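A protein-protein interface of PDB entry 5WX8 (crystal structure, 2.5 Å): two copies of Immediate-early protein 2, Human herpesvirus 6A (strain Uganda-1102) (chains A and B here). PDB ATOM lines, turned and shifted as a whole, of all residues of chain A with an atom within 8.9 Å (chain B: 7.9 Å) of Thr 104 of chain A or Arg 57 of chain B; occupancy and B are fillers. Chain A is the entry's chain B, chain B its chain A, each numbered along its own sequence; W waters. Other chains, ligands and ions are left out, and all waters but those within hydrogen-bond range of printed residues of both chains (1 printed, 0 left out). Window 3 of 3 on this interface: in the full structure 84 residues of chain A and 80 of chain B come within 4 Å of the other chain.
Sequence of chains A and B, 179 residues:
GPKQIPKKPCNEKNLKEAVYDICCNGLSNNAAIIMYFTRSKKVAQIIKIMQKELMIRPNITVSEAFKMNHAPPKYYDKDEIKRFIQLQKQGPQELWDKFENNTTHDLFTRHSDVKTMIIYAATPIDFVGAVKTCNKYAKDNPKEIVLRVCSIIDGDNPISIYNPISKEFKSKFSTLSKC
Among the printed residues, pairs that only touch across the chains: His 70 of chain A with Ile 60 of chain B (3.2 Å), His 70 of chain A with Thr 61 of chain B (3.6 Å), Ala 71 of chain A with Met 55 of chain B (3.8 Å), Ala 71 of chain A with Arg 57 of chain B (3.2 Å), Ala 71 of chain A with Pro 58 of chain B (3.7 Å), Ala 71 of chain A with Asn 59 of chain B (3.99 Å), Pro 72 of chain A with Pro 58 of chain B (3.1 Å), Pro 73 of chain A with Asn 59 of chain B (3.2 Å), Pro 73 of chain A with Tyr 162 of chain B (3.7 Å), Lys 74 of chain A with Pro 58 of chain B (3.8 Å), Tyr 76 of chain A with Asn 59 of chain B (3.5 Å), Tyr 76 of chain A with Ile 125 of chain B (3.5 Å), Phe 99 of chain A with Ile 125 of chain B (3.2 Å), Phe 99 of chain A with Gly 129 of chain B (3.5 Å), Asn 101 of chain A with Ile 125 of chain B (3.7 Å), Asn 102 of chain A with Arg 57 of chain B (3.8 Å), Thr 103 of chain A with Ile 56 of chain B (3.8 Å), Thr 103 of chain A with Pro 58 of chain B (3.7 Å), Thr 104 of chain A with Ile 56 of chain B (3.5 Å), Thr 104 of chain A with Arg 57 of chain B (3.9 Å), His 105 of chain A with Ile 56 of chain B (3.5 Å), His 105 of chain A with Arg 57 of chain B (3.9 Å), His 105 of chain A with Pro 58 of chain B (3.7 Å) and Thr 109 of chain A with Met 55 of chain B (3.9 Å).
OH of Tyr 76 of chain A lies within hydrogen-bond range of ND2 of Asn 101 of chain A.
A ring nitrogen (ND1) of His 105 of chain A lies close to the backbone NH (N) of Leu 107 of chain A (3.5 Å).
Water W1 lies within hydrogen-bond range of O of Ile 56 of chain B (3.0 Å) and O of His 105 of chain A (3.1 Å).
No position is printed for both chains.
Of the 34 pairs that touch across the chains among the printed residues, none has its exchanged pair printed and touching as well.
Of the printed residues of chain B, Asn 102 of chain A touches Arg 57 (3.8 Å).
Of the printed residues of chain B, Thr 103 of chain A touches Ile 56 (3.8 Å), Arg 57 (3.2 Å) and Pro 58 (3.7 Å).
Thr 104 of chain A touches just these residues of chain B: Ile 56 and Arg 57.
Of chain A, only Ala 71 (3.2 Å), Asn 101 (3.4 Å), Asn 102 (3.8 Å), Thr 103 (3.2 Å), Thr 104 (3.9 Å) and His 105 (3.9 Å) come within 4 Å of Arg 57 of chain B.
The nearest residue of chain A that does not touch Arg 57 of chain B is Pro 72 of chain A (5.3 Å).
The side-chain hydroxyl (OH) of Tyr 76 of chain A is in hydrogen-bond range of the side-chain carboxylate (OD1) of Asp 126 of chain B (2.7 Å).
O of Thr 103 of chain A is in hydrogen-bond range of NH1 of Arg 57 of chain B (3.2 Å).
O of Met 55 of chain B sits at hydrogen-bond distance from NE2 of His 105 of chain A (2.8 Å).
The backbone carbonyl oxygen (O) of Asn 101 of chain A sits close to the guanidinium group (NE) of Arg 57 of chain B, 3.4 Å away.
N of Lys 74 of chain A sits at hydrogen-bond distance from OD1 of Asn 59 of chain B, at 2.8 Å.
O of Ile 60 of chain B lies within hydrogen-bond range of N of Ala 71 of chain A, 2.9 Å away.
OH of Tyr 162 of chain B lies within hydrogen-bond range of ND1 of His 70 of chain A (3.1 Å).
The side-chain sulfur of Met 55 of chain B sits at hydrogen-bond distance from the backbone NH of His 70 of chain A.
The side-chain hydroxyl of Tyr 162 of chain B sits at hydrogen-bond distance from the backbone carbonyl oxygen of Ala 71 of chain A (2.7 Å).
The backbone carbonyl oxygen (O) of Pro 72 of chain A sits at hydrogen-bond distance from the backbone NH (N) of Asn 59 of chain B.
Of the 17 printed residues of chain A, 13 touch a printed residue of chain B.
Printed residues of chain B that touch a printed residue of chain A: Met 55, Ile 56, Arg 57, Pro 58, Asn 59, Ile 60, Thr 61, Ile 125, Asp 126, Gly 129 and Tyr 162.
Hydrophobic or aromatic side chains of chain B that line the printed part of chain A: Met 55, Pro 58, Ile 125 and Tyr 162.
Among the printed residues, no Asp or Glu carboxylate lies within 4 Å of a Lys or Arg side-chain nitrogen of the other chain.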
ATOM      1  N   HIS A  70       7.165 -21.454 -17.806  1.00  0.00           N
ATOM      2  CA  HIS A  70       7.991 -20.260 -17.654  1.00  0.00           C
ATOM      3  C   HIS A  70       7.723 -19.570 -16.324  1.00  0.00           C
ATOM      4  O   HIS A  70       6.695 -19.783 -15.675  1.00  0.00           O
ATOM      5  CB  HIS A  70       7.743 -19.269 -18.788  1.00  0.00           C
ATOM      6  CG  HIS A  70       6.397 -18.626 -18.734  1.00  0.00           C
ATOM      7  ND1 HIS A  70       6.164 -17.444 -18.062  1.00  0.00           N
ATOM      8  CD2 HIS A  70       5.213 -18.992 -19.273  1.00  0.00           C
ATOM      9  CE1 HIS A  70       4.896 -17.104 -18.199  1.00  0.00           C
ATOM     10  NE2 HIS A  70       4.298 -18.024 -18.934  1.00  0.00           N
ATOM     11  N   ALA A  71       8.658 -18.698 -15.964  1.00  0.00           N
ATOM     12  CA  ALA A  71       8.670 -17.956 -14.708  1.00  0.00           C
ATOM     13  C   ALA A  71       7.949 -16.619 -14.867  1.00  0.00           C
ATOM     14  O   ALA A  71       7.497 -16.257 -15.964  1.00  0.00           O
ATOM     15  CB  ALA A  71      10.117 -17.757 -14.266  1.00  0.00           C
ATOM     16  N   PRO A  72       7.788 -15.855 -13.778  1.00  0.00           N
ATOM     17  CA  PRO A  72       7.292 -14.488 -13.928  1.00  0.00           C
ATOM     18  C   PRO A  72       8.315 -13.625 -14.623  1.00  0.00           C
ATOM     19  O   PRO A  72       9.531 -13.900 -14.571  1.00  0.00           O
ATOM     20  CB  PRO A  72       7.068 -14.030 -12.472  1.00  0.00           C
ATOM     21  CG  PRO A  72       6.915 -15.292 -11.687  1.00  0.00           C
ATOM     22  CD  PRO A  72       7.856 -16.249 -12.360  1.00  0.00           C
ATOM     23  N   PRO A  73       7.891 -12.551 -15.291  1.00  0.00           N
ATOM     24  CA  PRO A  73       8.836 -11.627 -15.915  1.00  0.00           C
ATOM     25  C   PRO A  73       9.397 -10.634 -14.904  1.00  0.00           C
ATOM     26  O   PRO A  73       8.833 -10.411 -13.832  1.00  0.00           O
ATOM     27  CB  PRO A  73       7.986 -10.926 -16.987  1.00  0.00           C
ATOM     28  CG  PRO A  73       6.573 -10.984 -16.475  1.00  0.00           C
ATOM     29  CD  PRO A  73       6.480 -12.167 -15.526  1.00  0.00           C
ATOM     30  N   LYS A  74      10.563 -10.079 -15.237  1.00  0.00           N
ATOM     31  CA  LYS A  74      11.172  -9.043 -14.411  1.00  0.00           C
ATOM     32  C   LYS A  74      11.839  -7.982 -15.277  1.00  0.00           C
ATOM     33  O   LYS A  74      12.607  -8.307 -16.187  1.00  0.00           O
ATOM     34  CB  LYS A  74      12.202  -9.614 -13.449  1.00  0.00           C
ATOM     35  CG  LYS A  74      12.906  -8.513 -12.695  1.00  0.00           C
ATOM     36  CD  LYS A  74      13.980  -9.052 -11.787  1.00  0.00           C
ATOM     37  CE  LYS A  74      14.855  -7.921 -11.224  1.00  0.00           C
ATOM     38  NZ  LYS A  74      14.086  -6.808 -10.572  1.00  0.00           N
ATOM     39  N   TYR A  76      14.648  -5.329 -15.465  1.00  0.00           N
ATOM     40  CA  TYR A  76      15.868  -5.068 -14.732  1.00  0.00           C
ATOM     41  C   TYR A  76      16.111  -3.574 -14.594  1.00  0.00           C
ATOM     42  O   TYR A  76      15.785  -2.769 -15.470  1.00  0.00           O
ATOM     43  CB  TYR A  76      17.053  -5.757 -15.393  1.00  0.00           C
ATOM     44  CG  TYR A  76      17.087  -7.212 -15.023  1.00  0.00           C
ATOM     45  CD1 TYR A  76      17.492  -7.606 -13.750  1.00  0.00           C
ATOM     46  CD2 TYR A  76      16.667  -8.195 -15.926  1.00  0.00           C
ATOM     47  CE1 TYR A  76      17.513  -8.954 -13.386  1.00  0.00           C
ATOM     48  CE2 TYR A  76      16.687  -9.544 -15.583  1.00  0.00           C
ATOM     49  CZ  TYR A  76      17.106  -9.920 -14.305  1.00  0.00           C
ATOM     50  OH  TYR A  76      17.120 -11.248 -13.936  1.00  0.00           O
ATOM     51  N   GLU A  80      21.206  -2.151 -12.395  1.00  0.00           N
ATOM     52  CA  GLU A  80      21.606  -3.550 -12.527  1.00  0.00           C
ATOM     53  C   GLU A  80      22.141  -3.846 -13.927  1.00  0.00           C
ATOM     54  O   GLU A  80      23.094  -4.619 -14.084  1.00  0.00           O
ATOM     55  CB  GLU A  80      20.429  -4.474 -12.210  1.00  0.00           C
ATOM     56  CG  GLU A  80      20.271  -4.862 -10.744  1.00  0.00           C
ATOM     57  CD  GLU A  80      18.932  -5.545 -10.477  1.00  0.00           C
ATOM     58  OE1 GLU A  80      17.919  -5.133 -11.093  1.00  0.00           O
ATOM     59  OE2 GLU A  80      18.899  -6.495  -9.657  1.00  0.00           O
ATOM     60  N   PHE A  99      29.849 -13.488 -12.998  1.00  0.00           N
ATOM     61  CA  PHE A  99      28.417 -13.236 -12.995  1.00  0.00           C
ATOM     62  C   PHE A  99      27.745 -13.965 -11.837  1.00  0.00           C
ATOM     63  O   PHE A  99      28.042 -15.133 -11.554  1.00  0.00           O
ATOM     64  CB  PHE A  99      27.788 -13.654 -14.321  1.00  0.00           C
ATOM     65  CG  PHE A  99      26.312 -13.501 -14.345  1.00  0.00           C
ATOM     66  CD1 PHE A  99      25.730 -12.295 -14.686  1.00  0.00           C
ATOM     67  CD2 PHE A  99      25.498 -14.549 -13.988  1.00  0.00           C
ATOM     68  CE1 PHE A  99      24.349 -12.154 -14.682  1.00  0.00           C
ATOM     69  CE2 PHE A  99      24.123 -14.405 -13.989  1.00  0.00           C
ATOM     70  CZ  PHE A  99      23.553 -13.214 -14.340  1.00  0.00           C
ATOM     71  N   GLU A 100      26.864 -13.256 -11.149  1.00  0.00           N
ATOM     72  CA  GLU A 100      26.007 -13.851 -10.146  1.00  0.00           C
ATOM     73  C   GLU A 100      24.667 -13.154 -10.248  1.00  0.00           C
ATOM     74  O   GLU A 100      24.583 -11.981 -10.628  1.00  0.00           O
ATOM     75  CB  GLU A 100      26.592 -13.744  -8.724  1.00  0.00           C
ATOM     76  CG  GLU A 100      27.503 -14.939  -8.332  1.00  0.00           C
ATOM     77  CD  GLU A 100      28.591 -14.561  -7.327  1.00  0.00           C
ATOM     78  OE1 GLU A 100      29.757 -15.000  -7.497  1.00  0.00           O
ATOM     79  OE2 GLU A 100      28.274 -13.818  -6.369  1.00  0.00           O
ATOM     80  N   ASN A 101      23.618 -13.918  -9.979  1.00  0.00           N
ATOM     81  CA  ASN A 101      22.261 -13.396  -9.938  1.00  0.00           C
ATOM     82  C   ASN A 101      21.511 -14.131  -8.840  1.00  0.00           C
ATOM     83  O   ASN A 101      21.393 -15.364  -8.879  1.00  0.00           O
ATOM     84  CB  ASN A 101      21.544 -13.557 -11.275  1.00  0.00           C
ATOM     85  CG  ASN A 101      20.192 -12.885 -11.271  1.00  0.00           C
ATOM     86  OD1 ASN A 101      19.822 -12.232 -10.292  1.00  0.00           O
ATOM     87  ND2 ASN A 101      19.438 -13.045 -12.360  1.00  0.00           N
ATOM     88  N   ASN A 102      21.022 -13.365  -7.862  1.00  0.00           N
ATOM     89  CA  ASN A 102      20.265 -13.895  -6.737  1.00  0.00           C
ATOM     90  C   ASN A 102      18.824 -13.383  -6.726  1.00  0.00           C
ATOM     91  O   ASN A 102      18.222 -13.210  -5.666  1.00  0.00           O
ATOM     92  CB  ASN A 102      20.992 -13.562  -5.439  1.00  0.00           C
ATOM     93  CG  ASN A 102      22.328 -14.282  -5.333  1.00  0.00           C
ATOM     94  OD1 ASN A 102      22.374 -15.508  -5.150  1.00  0.00           O
ATOM     95  ND2 ASN A 102      23.424 -13.530  -5.463  1.00  0.00           N
ATOM     96  N   THR A 103      18.261 -13.161  -7.914  1.00  0.00           N
ATOM     97  CA  THR A 103      16.893 -12.686  -8.066  1.00  0.00           C
ATOM     98  C   THR A 103      15.905 -13.845  -7.974  1.00  0.00           C
ATOM     99  O   THR A 103      16.060 -14.864  -8.658  1.00  0.00           O
ATOM    100  CB  THR A 103      16.737 -11.977  -9.414  1.00  0.00           C
ATOM    101  OG1 THR A 103      17.731 -10.955  -9.551  1.00  0.00           O
ATOM    102  CG2 THR A 103      15.357 -11.379  -9.540  1.00  0.00           C
ATOM    103  N   THR A 104      14.884 -13.689  -7.143  1.00  0.00           N
ATOM    104  CA  THR A 104      13.806 -14.659  -7.023  1.00  0.00           C
ATOM    105  C   THR A 104      12.474 -13.984  -7.366  1.00  0.00           C
ATOM    106  O   THR A 104      12.427 -12.814  -7.746  1.00  0.00           O
ATOM    107  CB  THR A 104      13.787 -15.272  -5.617  1.00  0.00           C
ATOM    108  OG1 THR A 104      13.402 -14.276  -4.660  1.00  0.00           O
ATOM    109  CG2 THR A 104      15.160 -15.819  -5.256  1.00  0.00           C
ATOM    110  N   HIS A 105      11.385 -14.743  -7.247  1.00  0.00           N
ATOM    111  CA  HIS A 105      10.034 -14.222  -7.446  1.00  0.00           C
ATOM    112  C   HIS A 105       9.089 -15.008  -6.551  1.00  0.00           C
ATOM    113  O   HIS A 105       9.375 -16.145  -6.170  1.00  0.00           O
ATOM    114  CB  HIS A 105       9.585 -14.332  -8.903  1.00  0.00           C
ATOM    115  CG  HIS A 105       9.661 -15.726  -9.434  1.00  0.00           C
ATOM    116  ND1 HIS A 105       8.782 -16.716  -9.046  1.00  0.00           N
ATOM    117  CD2 HIS A 105      10.541 -16.310 -10.283  1.00  0.00           C
ATOM    118  CE1 HIS A 105       9.113 -17.844  -9.645  1.00  0.00           C
ATOM    119  NE2 HIS A 105      10.177 -17.627 -10.397  1.00  0.00           N
ATOM    120  N   ASP A 106       7.946 -14.406  -6.225  1.00  0.00           N
ATOM    121  CA  ASP A 106       7.050 -14.984  -5.228  1.00  0.00           C
ATOM    122  C   ASP A 106       5.889 -15.753  -5.839  1.00  0.00           C
ATOM    123  O   ASP A 106       4.914 -16.040  -5.141  1.00  0.00           O
ATOM    124  CB  ASP A 106       6.505 -13.896  -4.304  1.00  0.00           C
ATOM    125  CG  ASP A 106       7.503 -13.492  -3.252  1.00  0.00           C
ATOM    126  OD1 ASP A 106       8.082 -14.390  -2.593  1.00  0.00           O
ATOM    127  OD2 ASP A 106       7.724 -12.278  -3.097  1.00  0.00           O
ATOM    128  N   LEU A 107       5.972 -16.102  -7.113  1.00  0.00           N
ATOM    129  CA  LEU A 107       4.820 -16.628  -7.824  1.00  0.00           C
ATOM    130  C   LEU A 107       5.041 -18.092  -8.211  1.00  0.00           C
ATOM    131  O   LEU A 107       6.019 -18.737  -7.812  1.00  0.00           O
ATOM    132  CB  LEU A 107       4.534 -15.756  -9.046  1.00  0.00           C
ATOM    133  CG  LEU A 107       3.855 -14.422  -8.706  1.00  0.00           C
ATOM    134  CD1 LEU A 107       3.179 -13.850  -9.945  1.00  0.00           C
ATOM    135  CD2 LEU A 107       2.855 -14.606  -7.550  1.00  0.00           C
ATOM    136  N   THR A 109       5.041 -21.198 -11.336  1.00  0.00           N
ATOM    137  CA  THR A 109       5.313 -21.462 -12.739  1.00  0.00           C
ATOM    138  C   THR A 109       4.015 -21.470 -13.532  1.00  0.00           C
ATOM    139  O   THR A 109       2.993 -22.002 -13.089  1.00  0.00           O
ATOM    140  CB  THR A 109       6.042 -22.799 -12.882  1.00  0.00           C
ATOM    141  OG1 THR A 109       7.225 -22.782 -12.071  1.00  0.00           O
ATOM    142  CG2 THR A 109       6.440 -23.052 -14.328  1.00  0.00           C
ATOM    143  N   GLN B  51      14.545 -28.206 -14.035  1.00  0.00           N
ATOM    144  CA  GLN B  51      13.390 -27.361 -14.342  1.00  0.00           C
ATOM    145  C   GLN B  51      13.036 -26.478 -13.150  1.00  0.00           C
ATOM    146  O   GLN B  51      12.845 -25.261 -13.295  1.00  0.00           O
ATOM    147  CB  GLN B  51      12.181 -28.223 -14.746  1.00  0.00           C
ATOM    148  CG  GLN B  51      12.191 -28.763 -16.183  1.00  0.00           C
ATOM    149  CD  GLN B  51      11.167 -29.894 -16.411  1.00  0.00           C
ATOM    150  OE1 GLN B  51      10.684 -30.530 -15.454  1.00  0.00           O
ATOM    151  NE2 GLN B  51      10.851 -30.159 -17.685  1.00  0.00           N
ATOM    152  N   LYS B  52      12.978 -27.084 -11.954  1.00  0.00           N
ATOM    153  CA  LYS B  52      12.654 -26.351 -10.734  1.00  0.00           C
ATOM    154  C   LYS B  52      13.724 -25.311 -10.412  1.00  0.00           C
ATOM    155  O   LYS B  52      13.409 -24.136 -10.191  1.00  0.00           O
ATOM    156  CB  LYS B  52      12.468 -27.335  -9.565  1.00  0.00           C
ATOM    157  CG  LYS B  52      12.395 -26.704  -8.163  1.00  0.00           C
ATOM    158  CD  LYS B  52      12.644 -27.729  -7.017  1.00  0.00           C
ATOM    159  CE  LYS B  52      14.081 -28.333  -7.009  1.00  0.00           C
ATOM    160  NZ  LYS B  52      15.232 -27.338  -6.993  1.00  0.00           N
ATOM    161  N   GLU B  53      15.001 -25.724 -10.381  1.00  0.00           N
ATOM    162  CA  GLU B  53      16.072 -24.781 -10.048  1.00  0.00           C
ATOM    163  C   GLU B  53      16.139 -23.654 -11.071  1.00  0.00           C
ATOM    164  O   GLU B  53      16.353 -22.496 -10.710  1.00  0.00           O
ATOM    165  CB  GLU B  53      17.412 -25.508  -9.956  1.00  0.00           C
ATOM    166  CG  GLU B  53      18.651 -24.617  -9.737  1.00  0.00           C
ATOM    167  CD  GLU B  53      19.919 -25.443  -9.453  1.00  0.00           C
ATOM    168  OE1 GLU B  53      19.832 -26.692  -9.479  1.00  0.00           O
ATOM    169  OE2 GLU B  53      21.000 -24.854  -9.211  1.00  0.00           O
ATOM    170  N   LEU B  54      15.943 -23.983 -12.347  1.00  0.00           N
ATOM    171  CA  LEU B  54      16.026 -22.993 -13.414  1.00  0.00           C
ATOM    172  C   LEU B  54      14.978 -21.893 -13.249  1.00  0.00           C
ATOM    173  O   LEU B  54      15.237 -20.722 -13.555  1.00  0.00           O
ATOM    174  CB  LEU B  54      15.829 -23.696 -14.756  1.00  0.00           C
ATOM    175  CG  LEU B  54      16.798 -23.569 -15.920  1.00  0.00           C
ATOM    176  CD1 LEU B  54      18.212 -23.201 -15.463  1.00  0.00           C
ATOM    177  CD2 LEU B  54      16.768 -24.896 -16.696  1.00  0.00           C
ATOM    178  N   MET B  55      13.782 -22.255 -12.788  1.00  0.00           N
ATOM    179  CA  MET B  55      12.664 -21.330 -12.824  1.00  0.00           C
ATOM    180  C   MET B  55      12.357 -20.661 -11.472  1.00  0.00           C
ATOM    181  O   MET B  55      11.380 -19.928 -11.365  1.00  0.00           O
ATOM    182  CB  MET B  55      11.430 -22.045 -13.385  1.00  0.00           C
ATOM    183  CG  MET B  55      11.409 -21.919 -14.913  1.00  0.00           C
ATOM    184  SD  MET B  55       9.954 -22.782 -15.906  1.00  0.00           S
ATOM    185  CE  MET B  55      10.030 -24.549 -15.109  1.00  0.00           C
ATOM    186  N   ILE B  56      13.204 -20.867 -10.456  1.00  0.00           N
ATOM    187  CA  ILE B  56      13.190 -19.961  -9.314  1.00  0.00           C
ATOM    188  C   ILE B  56      13.672 -18.562  -9.685  1.00  0.00           C
ATOM    189  O   ILE B  56      13.473 -17.613  -8.907  1.00  0.00           O
ATOM    190  CB  ILE B  56      14.031 -20.518  -8.143  1.00  0.00           C
ATOM    191  CG1 ILE B  56      15.517 -20.204  -8.326  1.00  0.00           C
ATOM    192  CG2 ILE B  56      13.814 -22.001  -8.002  1.00  0.00           C
ATOM    193  CD1 ILE B  56      16.394 -20.750  -7.221  1.00  0.00           C
ATOM    194  N   ARG B  57      14.298 -18.408 -10.858  1.00  0.00           N
ATOM    195  CA  ARG B  57      14.707 -17.140 -11.446  1.00  0.00           C
ATOM    196  C   ARG B  57      13.697 -16.698 -12.494  1.00  0.00           C
ATOM    197  O   ARG B  57      13.188 -17.530 -13.248  1.00  0.00           O
ATOM    198  CB  ARG B  57      16.100 -17.243 -12.080  1.00  0.00           C
ATOM    199  CG  ARG B  57      17.134 -17.921 -11.165  1.00  0.00           C
ATOM    200  CD  ARG B  57      17.905 -16.962 -10.300  1.00  0.00           C
ATOM    201  NE  ARG B  57      18.951 -17.637  -9.529  1.00  0.00           N
ATOM    202  CZ  ARG B  57      19.034 -17.643  -8.191  1.00  0.00           C
ATOM    203  NH1 ARG B  57      18.132 -17.000  -7.448  1.00  0.00           N
ATOM    204  NH2 ARG B  57      20.030 -18.290  -7.585  1.00  0.00           N
ATOM    205  N   PRO B  58      13.368 -15.409 -12.519  1.00  0.00           N
ATOM    206  CA  PRO B  58      12.414 -14.895 -13.511  1.00  0.00           C
ATOM    207  C   PRO B  58      12.980 -14.892 -14.926  1.00  0.00           C
ATOM    208  O   PRO B  58      14.181 -15.058 -15.171  1.00  0.00           O
ATOM    209  CB  PRO B  58      12.150 -13.462 -13.041  1.00  0.00           C
ATOM    210  CG  PRO B  58      13.406 -13.078 -12.310  1.00  0.00           C
ATOM    211  CD  PRO B  58      13.874 -14.348 -11.633  1.00  0.00           C
ATOM    212  N   ASN B  59      12.069 -14.669 -15.869  1.00  0.00           N
ATOM    213  CA  ASN B  59      12.335 -14.520 -17.298  1.00  0.00           C
ATOM    214  C   ASN B  59      12.771 -15.805 -17.978  1.00  0.00           C
ATOM    215  O   ASN B  59      13.150 -15.762 -19.155  1.00  0.00           O
ATOM    216  CB  ASN B  59      13.399 -13.457 -17.590  1.00  0.00           C
ATOM    217  CG  ASN B  59      12.948 -12.066 -17.231  1.00  0.00           C
ATOM    218  OD1 ASN B  59      11.742 -11.792 -17.158  1.00  0.00           O
ATOM    219  ND2 ASN B  59      13.915 -11.170 -16.996  1.00  0.00           N
ATOM    220  N   ILE B  60      12.750 -16.942 -17.287  1.00  0.00           N
ATOM    221  CA  ILE B  60      13.204 -18.197 -17.869  1.00  0.00           C
ATOM    222  C   ILE B  60      12.016 -19.006 -18.349  1.00  0.00           C
ATOM    223  O   ILE B  60      11.042 -19.214 -17.615  1.00  0.00           O
ATOM    224  CB  ILE B  60      14.033 -19.019 -16.883  1.00  0.00           C
ATOM    225  CG1 ILE B  60      15.236 -18.211 -16.436  1.00  0.00           C
ATOM    226  CG2 ILE B  60      14.449 -20.317 -17.533  1.00  0.00           C
ATOM    227  CD1 ILE B  60      16.047 -17.704 -17.585  1.00  0.00           C
ATOM    228  N   THR B  61      12.118 -19.486 -19.579  1.00  0.00           N
ATOM    229  CA  THR B  61      11.233 -20.505 -20.084  1.00  0.00           C
ATOM    230  C   THR B  61      11.937 -21.844 -20.275  1.00  0.00           C
ATOM    231  O   THR B  61      12.947 -21.914 -20.974  1.00  0.00           O
ATOM    232  CB  THR B  61      10.649 -20.097 -21.403  1.00  0.00           C
ATOM    233  OG1 THR B  61      10.199 -18.743 -21.337  1.00  0.00           O
ATOM    234  CG2 THR B  61       9.392 -20.863 -21.725  1.00  0.00           C
ATOM    235  N   TYR B 120      14.852 -21.024 -22.574  1.00  0.00           N
ATOM    236  CA  TYR B 120      15.011 -19.655 -23.059  1.00  0.00           C
ATOM    237  C   TYR B 120      15.095 -18.674 -21.892  1.00  0.00           C
ATOM    238  O   TYR B 120      14.759 -18.994 -20.750  1.00  0.00           O
ATOM    239  CB  TYR B 120      13.876 -19.209 -23.978  1.00  0.00           C
ATOM    240  CG  TYR B 120      13.410 -20.204 -24.998  1.00  0.00           C
ATOM    241  CD1 TYR B 120      12.429 -21.131 -24.676  1.00  0.00           C
ATOM    242  CD2 TYR B 120      13.898 -20.202 -26.303  1.00  0.00           C
ATOM    243  CE1 TYR B 120      11.968 -22.048 -25.610  1.00  0.00           C
ATOM    244  CE2 TYR B 120      13.420 -21.118 -27.250  1.00  0.00           C
ATOM    245  CZ  TYR B 120      12.446 -22.032 -26.878  1.00  0.00           C
ATOM    246  OH  TYR B 120      11.920 -22.948 -27.746  1.00  0.00           O
ATOM    247  N   ILE B 125      20.996 -11.088 -18.881  1.00  0.00           N
ATOM    248  CA  ILE B 125      21.214 -11.422 -17.470  1.00  0.00           C
ATOM    249  C   ILE B 125      20.647 -12.807 -17.152  1.00  0.00           C
ATOM    250  O   ILE B 125      21.304 -13.648 -16.528  1.00  0.00           O
ATOM    251  CB  ILE B 125      20.597 -10.343 -16.561  1.00  0.00           C
ATOM    252  CG1 ILE B 125      21.483  -9.096 -16.511  1.00  0.00           C
ATOM    253  CG2 ILE B 125      20.426 -10.880 -15.169  1.00  0.00           C
ATOM    254  CD1 ILE B 125      20.910  -7.972 -15.681  1.00  0.00           C
ATOM    255  N   ASP B 126      19.415 -13.065 -17.582  1.00  0.00           N
ATOM    256  CA  ASP B 126      18.818 -14.363 -17.318  1.00  0.00           C
ATOM    257  C   ASP B 126      19.531 -15.465 -18.091  1.00  0.00           C
ATOM    258  O   ASP B 126      19.646 -16.601 -17.606  1.00  0.00           O
ATOM    259  CB  ASP B 126      17.336 -14.304 -17.675  1.00  0.00           C
ATOM    260  CG  ASP B 126      16.664 -13.054 -17.126  1.00  0.00           C
ATOM    261  OD1 ASP B 126      16.472 -13.009 -15.893  1.00  0.00           O
ATOM    262  OD2 ASP B 126      16.357 -12.121 -17.907  1.00  0.00           O
ATOM    263  N   GLY B 129      23.008 -16.640 -16.418  1.00  0.00           N
ATOM    264  CA  GLY B 129      22.675 -17.403 -15.226  1.00  0.00           C
ATOM    265  C   GLY B 129      21.954 -18.713 -15.496  1.00  0.00           C
ATOM    266  O   GLY B 129      22.021 -19.629 -14.662  1.00  0.00           O
ATOM    267  N   ALA B 130      21.279 -18.833 -16.638  1.00  0.00           N
ATOM    268  CA  ALA B 130      20.653 -20.111 -16.963  1.00  0.00           C
ATOM    269  C   ALA B 130      21.659 -21.089 -17.554  1.00  0.00           C
ATOM    270  O   ALA B 130      21.618 -22.290 -17.256  1.00  0.00           O
ATOM    271  CB  ALA B 130      19.492 -19.903 -17.933  1.00  0.00           C
ATOM    272  N   THR B 133      23.818 -22.543 -14.821  1.00  0.00           N
ATOM    273  CA  THR B 133      23.122 -23.589 -14.079  1.00  0.00           C
ATOM    274  C   THR B 133      23.096 -24.897 -14.864  1.00  0.00           C
ATOM    275  O   THR B 133      23.372 -25.970 -14.318  1.00  0.00           O
ATOM    276  CB  THR B 133      21.701 -23.130 -13.741  1.00  0.00           C
ATOM    277  OG1 THR B 133      21.752 -22.192 -12.657  1.00  0.00           O
ATOM    278  CG2 THR B 133      20.831 -24.327 -13.355  1.00  0.00           C
ATOM    279  N   TYR B 162       7.040 -11.637 -22.484  1.00  0.00           N
ATOM    280  CA  TYR B 162       8.393 -11.201 -22.159  1.00  0.00           C
ATOM    281  C   TYR B 162       8.885 -10.085 -23.069  1.00  0.00           C
ATOM    282  O   TYR B 162       9.881  -9.428 -22.743  1.00  0.00           O
ATOM    283  CB  TYR B 162       9.363 -12.382 -22.262  1.00  0.00           C
ATOM    284  CG  TYR B 162       9.277 -13.412 -21.152  1.00  0.00           C
ATOM    285  CD1 TYR B 162       9.254 -13.032 -19.808  1.00  0.00           C
ATOM    286  CD2 TYR B 162       9.243 -14.772 -21.450  1.00  0.00           C
ATOM    287  CE1 TYR B 162       9.184 -13.989 -18.794  1.00  0.00           C
ATOM    288  CE2 TYR B 162       9.180 -15.727 -20.454  1.00  0.00           C
ATOM    289  CZ  TYR B 162       9.148 -15.339 -19.137  1.00  0.00           C
ATOM    290  OH  TYR B 162       9.092 -16.311 -18.166  1.00  0.00           O
HETATM  291  O   HOH W   1      11.652 -18.207  -6.628  1.00  0.00           O
